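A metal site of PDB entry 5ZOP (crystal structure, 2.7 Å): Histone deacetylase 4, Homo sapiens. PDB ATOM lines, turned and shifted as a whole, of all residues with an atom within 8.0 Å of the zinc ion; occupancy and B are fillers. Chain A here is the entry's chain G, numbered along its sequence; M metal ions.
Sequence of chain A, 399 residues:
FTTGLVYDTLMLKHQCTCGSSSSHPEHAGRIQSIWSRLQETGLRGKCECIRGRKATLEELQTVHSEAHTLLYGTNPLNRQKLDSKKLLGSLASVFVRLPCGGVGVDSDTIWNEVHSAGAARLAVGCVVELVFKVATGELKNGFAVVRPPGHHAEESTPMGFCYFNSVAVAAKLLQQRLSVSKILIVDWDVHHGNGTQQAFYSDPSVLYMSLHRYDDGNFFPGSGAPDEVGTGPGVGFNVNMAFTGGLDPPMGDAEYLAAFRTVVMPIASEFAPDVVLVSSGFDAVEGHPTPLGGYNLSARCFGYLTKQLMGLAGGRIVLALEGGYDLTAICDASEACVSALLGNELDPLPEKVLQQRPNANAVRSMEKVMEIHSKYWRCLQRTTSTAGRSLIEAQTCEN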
ATOM      1  N   GLN A  15     -34.939  18.434 -28.897  1.00  0.00           N
ATOM      2  CA  GLN A  15     -33.859  17.725 -29.559  1.00  0.00           C
ATOM      3  C   GLN A  15     -32.538  18.141 -28.920  1.00  0.00           C
ATOM      4  O   GLN A  15     -32.368  19.285 -28.499  1.00  0.00           O
ATOM      5  CB  GLN A  15     -33.862  18.029 -31.059  1.00  0.00           C
ATOM      6  CG  GLN A  15     -32.847  17.258 -31.871  1.00  0.00           C
ATOM      7  CD  GLN A  15     -33.006  17.492 -33.365  1.00  0.00           C
ATOM      8  OE1 GLN A  15     -33.805  16.834 -34.029  1.00  0.00           O
ATOM      9  NE2 GLN A  15     -32.236  18.445 -33.892  1.00  0.00           N
ATOM     10  N   CYS A  16     -31.612  17.182 -28.851  1.00  0.00           N
ATOM     11  CA  CYS A  16     -30.306  17.459 -28.274  1.00  0.00           C
ATOM     12  C   CYS A  16     -29.465  18.317 -29.222  1.00  0.00           C
ATOM     13  O   CYS A  16     -29.559  18.224 -30.449  1.00  0.00           O
ATOM     14  CB  CYS A  16     -29.570  16.161 -27.970  1.00  0.00           C
ATOM     15  SG  CYS A  16     -28.027  16.399 -27.052  1.00  0.00           S
ATOM     16  N   THR A  17     -28.627  19.164 -28.622  1.00  0.00           N
ATOM     17  CA  THR A  17     -27.772  20.078 -29.383  1.00  0.00           C
ATOM     18  C   THR A  17     -26.558  19.387 -30.005  1.00  0.00           C
ATOM     19  O   THR A  17     -25.910  19.988 -30.863  1.00  0.00           O
ATOM     20  CB  THR A  17     -27.298  21.215 -28.480  1.00  0.00           C
ATOM     21  OG1 THR A  17     -26.486  20.687 -27.432  1.00  0.00           O
ATOM     22  CG2 THR A  17     -28.489  21.937 -27.873  1.00  0.00           C
ATOM     23  N   CYS A  18     -26.238  18.161 -29.583  1.00  0.00           N
ATOM     24  CA  CYS A  18     -24.996  17.528 -30.020  1.00  0.00           C
ATOM     25  C   CYS A  18     -24.966  17.259 -31.519  1.00  0.00           C
ATOM     26  O   CYS A  18     -23.890  17.249 -32.130  1.00  0.00           O
ATOM     27  CB  CYS A  18     -24.772  16.229 -29.247  1.00  0.00           C
ATOM     28  SG  CYS A  18     -25.935  14.897 -29.667  1.00  0.00           S
ATOM     29  N   GLY A  19     -26.124  17.028 -32.130  1.00  0.00           N
ATOM     30  CA  GLY A  19     -26.166  16.652 -33.523  1.00  0.00           C
ATOM     31  C   GLY A  19     -25.907  15.173 -33.800  1.00  0.00           C
ATOM     32  O   GLY A  19     -25.707  14.812 -34.967  1.00  0.00           O
ATOM     33  N   SER A  20     -25.889  14.339 -32.775  1.00  0.00           N
ATOM     34  CA  SER A  20     -25.730  12.894 -32.928  1.00  0.00           C
ATOM     35  C   SER A  20     -27.093  12.238 -32.701  1.00  0.00           C
ATOM     36  O   SER A  20     -27.480  11.976 -31.561  1.00  0.00           O
ATOM     37  CB  SER A  20     -24.684  12.350 -31.964  1.00  0.00           C
ATOM     38  OG  SER A  20     -24.428  10.972 -32.184  1.00  0.00           O
ATOM     39  N   SER A  21     -27.810  11.985 -33.790  1.00  0.00           N
ATOM     40  CA  SER A  21     -29.140  11.387 -33.682  1.00  0.00           C
ATOM     41  C   SER A  21     -29.076   9.954 -33.163  1.00  0.00           C
ATOM     42  O   SER A  21     -30.042   9.471 -32.557  1.00  0.00           O
ATOM     43  CB  SER A  21     -29.838  11.423 -35.038  1.00  0.00           C
ATOM     44  OG  SER A  21     -29.862  12.732 -35.577  1.00  0.00           O
ATOM     45  N   SER A  23     -27.395   8.650 -30.752  1.00  0.00           N
ATOM     46  CA  SER A  23     -27.204   8.496 -29.316  1.00  0.00           C
ATOM     47  C   SER A  23     -28.479   8.678 -28.502  1.00  0.00           C
ATOM     48  O   SER A  23     -28.479   8.381 -27.305  1.00  0.00           O
ATOM     49  CB  SER A  23     -26.154   9.495 -28.814  1.00  0.00           C
ATOM     50  OG  SER A  23     -24.958   9.383 -29.570  1.00  0.00           O
ATOM     51  N   HIS A  24     -29.565   9.155 -29.113  1.00  0.00           N
ATOM     52  CA  HIS A  24     -30.805   9.460 -28.400  1.00  0.00           C
ATOM     53  C   HIS A  24     -31.965   8.750 -29.070  1.00  0.00           C
ATOM     54  O   HIS A  24     -32.548   9.265 -30.040  1.00  0.00           O
ATOM     55  CB  HIS A  24     -31.026  10.967 -28.322  1.00  0.00           C
ATOM     56  CG  HIS A  24     -29.837  11.720 -27.809  1.00  0.00           C
ATOM     57  ND1 HIS A  24     -29.202  11.387 -26.633  1.00  0.00           N
ATOM     58  CD2 HIS A  24     -29.148  12.762 -28.329  1.00  0.00           C
ATOM     59  CE1 HIS A  24     -28.184  12.196 -26.442  1.00  0.00           C
ATOM     60  NE2 HIS A  24     -28.129  13.040 -27.458  1.00  0.00           N
ATOM     61  N   LEU A  98     -23.214  16.536 -20.849  1.00  0.00           N
ATOM     62  CA  LEU A  98     -23.249  15.139 -21.249  1.00  0.00           C
ATOM     63  C   LEU A  98     -22.025  14.764 -22.078  1.00  0.00           C
ATOM     64  O   LEU A  98     -21.393  15.619 -22.692  1.00  0.00           O
ATOM     65  CB  LEU A  98     -24.522  14.853 -22.042  1.00  0.00           C
ATOM     66  CG  LEU A  98     -25.826  15.052 -21.265  1.00  0.00           C
ATOM     67  CD1 LEU A  98     -27.025  14.674 -22.116  1.00  0.00           C
ATOM     68  CD2 LEU A  98     -25.787  14.256 -19.971  1.00  0.00           C
ATOM     69  N   PRO A  99     -21.669  13.468 -22.093  1.00  0.00           N
ATOM     70  CA  PRO A  99     -20.569  13.027 -22.983  1.00  0.00           C
ATOM     71  C   PRO A  99     -20.831  13.321 -24.444  1.00  0.00           C
ATOM     72  O   PRO A  99     -19.870  13.542 -25.200  1.00  0.00           O
ATOM     73  CB  PRO A  99     -20.489  11.518 -22.706  1.00  0.00           C
ATOM     74  CG  PRO A  99     -21.069  11.352 -21.340  1.00  0.00           C
ATOM     75  CD  PRO A  99     -22.151  12.382 -21.238  1.00  0.00           C
ATOM     76  N   CYS A 100     -22.086  13.317 -24.889  1.00  0.00           N
ATOM     77  CA  CYS A 100     -22.402  13.677 -26.264  1.00  0.00           C
ATOM     78  C   CYS A 100     -22.104  15.147 -26.553  1.00  0.00           C
ATOM     79  O   CYS A 100     -21.936  15.509 -27.726  1.00  0.00           O
ATOM     80  CB  CYS A 100     -23.873  13.379 -26.564  1.00  0.00           C
ATOM     81  SG  CYS A 100     -25.047  14.383 -25.617  1.00  0.00           S
ATOM     82  N   GLY A 101     -22.029  15.988 -25.519  1.00  0.00           N
ATOM     83  CA  GLY A 101     -21.808  17.409 -25.683  1.00  0.00           C
ATOM     84  C   GLY A 101     -23.025  18.282 -25.463  1.00  0.00           C
ATOM     85  O   GLY A 101     -22.878  19.501 -25.325  1.00  0.00           O
ATOM     86  N   GLY A 102     -24.226  17.697 -25.446  1.00  0.00           N
ATOM     87  CA  GLY A 102     -25.405  18.457 -25.105  1.00  0.00           C
ATOM     88  C   GLY A 102     -25.604  18.577 -23.605  1.00  0.00           C
ATOM     89  O   GLY A 102     -24.943  17.924 -22.802  1.00  0.00           O
ATOM     90  N   VAL A 103     -26.533  19.454 -23.235  1.00  0.00           N
ATOM     91  CA  VAL A 103     -26.952  19.587 -21.844  1.00  0.00           C
ATOM     92  C   VAL A 103     -27.967  18.499 -21.518  1.00  0.00           C
ATOM     93  O   VAL A 103     -28.679  17.996 -22.394  1.00  0.00           O
ATOM     94  CB  VAL A 103     -27.537  20.996 -21.588  1.00  0.00           C
ATOM     95  CG1 VAL A 103     -27.600  21.290 -20.095  1.00  0.00           C
ATOM     96  CG2 VAL A 103     -26.708  22.051 -22.311  1.00  0.00           C
ATOM     97  N   SER A 107     -27.574  10.845 -18.360  1.00  0.00           N
ATOM     98  CA  SER A 107     -27.159  10.321 -19.662  1.00  0.00           C
ATOM     99  C   SER A 107     -28.337  10.044 -20.581  1.00  0.00           C
ATOM    100  O   SER A 107     -28.211  10.150 -21.808  1.00  0.00           O
ATOM    101  CB  SER A 107     -26.317   9.063 -19.477  1.00  0.00           C
ATOM    102  OG  SER A 107     -27.003   8.099 -18.688  1.00  0.00           O
ATOM    103  N   ILE A 110     -31.834  14.163 -22.275  1.00  0.00           N
ATOM    104  CA  ILE A 110     -31.251  15.407 -22.758  1.00  0.00           C
ATOM    105  C   ILE A 110     -32.215  16.568 -22.536  1.00  0.00           C
ATOM    106  O   ILE A 110     -33.439  16.388 -22.492  1.00  0.00           O
ATOM    107  CB  ILE A 110     -30.859  15.269 -24.235  1.00  0.00           C
ATOM    108  CG1 ILE A 110     -32.089  14.915 -25.082  1.00  0.00           C
ATOM    109  CG2 ILE A 110     -29.798  14.206 -24.403  1.00  0.00           C
ATOM    110  CD1 ILE A 110     -32.732  16.094 -25.778  1.00  0.00           C
ATOM    111  N   TRP A 111     -31.658  17.774 -22.417  1.00  0.00           N
ATOM    112  CA  TRP A 111     -32.460  18.977 -22.181  1.00  0.00           C
ATOM    113  C   TRP A 111     -31.992  20.088 -23.106  1.00  0.00           C
ATOM    114  O   TRP A 111     -30.866  20.588 -22.978  1.00  0.00           O
ATOM    115  CB  TRP A 111     -32.373  19.417 -20.726  1.00  0.00           C
ATOM    116  CG  TRP A 111     -33.089  20.689 -20.444  1.00  0.00           C
ATOM    117  CD1 TRP A 111     -32.538  21.937 -20.326  1.00  0.00           C
ATOM    118  CD2 TRP A 111     -34.495  20.860 -20.268  1.00  0.00           C
ATOM    119  NE1 TRP A 111     -33.519  22.862 -20.071  1.00  0.00           N
ATOM    120  CE2 TRP A 111     -34.732  22.227 -20.029  1.00  0.00           C
ATOM    121  CE3 TRP A 111     -35.585  19.983 -20.273  1.00  0.00           C
ATOM    122  CZ2 TRP A 111     -36.006  22.736 -19.806  1.00  0.00           C
ATOM    123  CZ3 TRP A 111     -36.860  20.492 -20.059  1.00  0.00           C
ATOM    124  CH2 TRP A 111     -37.056  21.864 -19.828  1.00  0.00           C
HETATM  125 ZN    ZN M   1     -26.682  14.590 -27.412  1.00  0.00          ZN
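Of the 18 residues printed, 4 come within 4 Å of the zinc ion.
NE2 of His 24 binds the zinc ion, at 2.1 Å. The zinc ion is bound by the side-chain sulfur (SG) of Cys 16, at 2.3 Å. SG of Cys 18 is bound to the zinc ion, 2.4 Å away. The zinc ion is bound by the side-chain sulfur (SG) of Cys 100. The zinc ion has four donor atoms within binding distance.
The side-chain sulfur (SG) of Cys 18 lies close to the backbone NH (N) of Ser 20, 3.2 Å away. The side-chain sulfur (SG) of Cys 100 lies close to the backbone NH (N) of Gly 102, 3.4 Å away.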
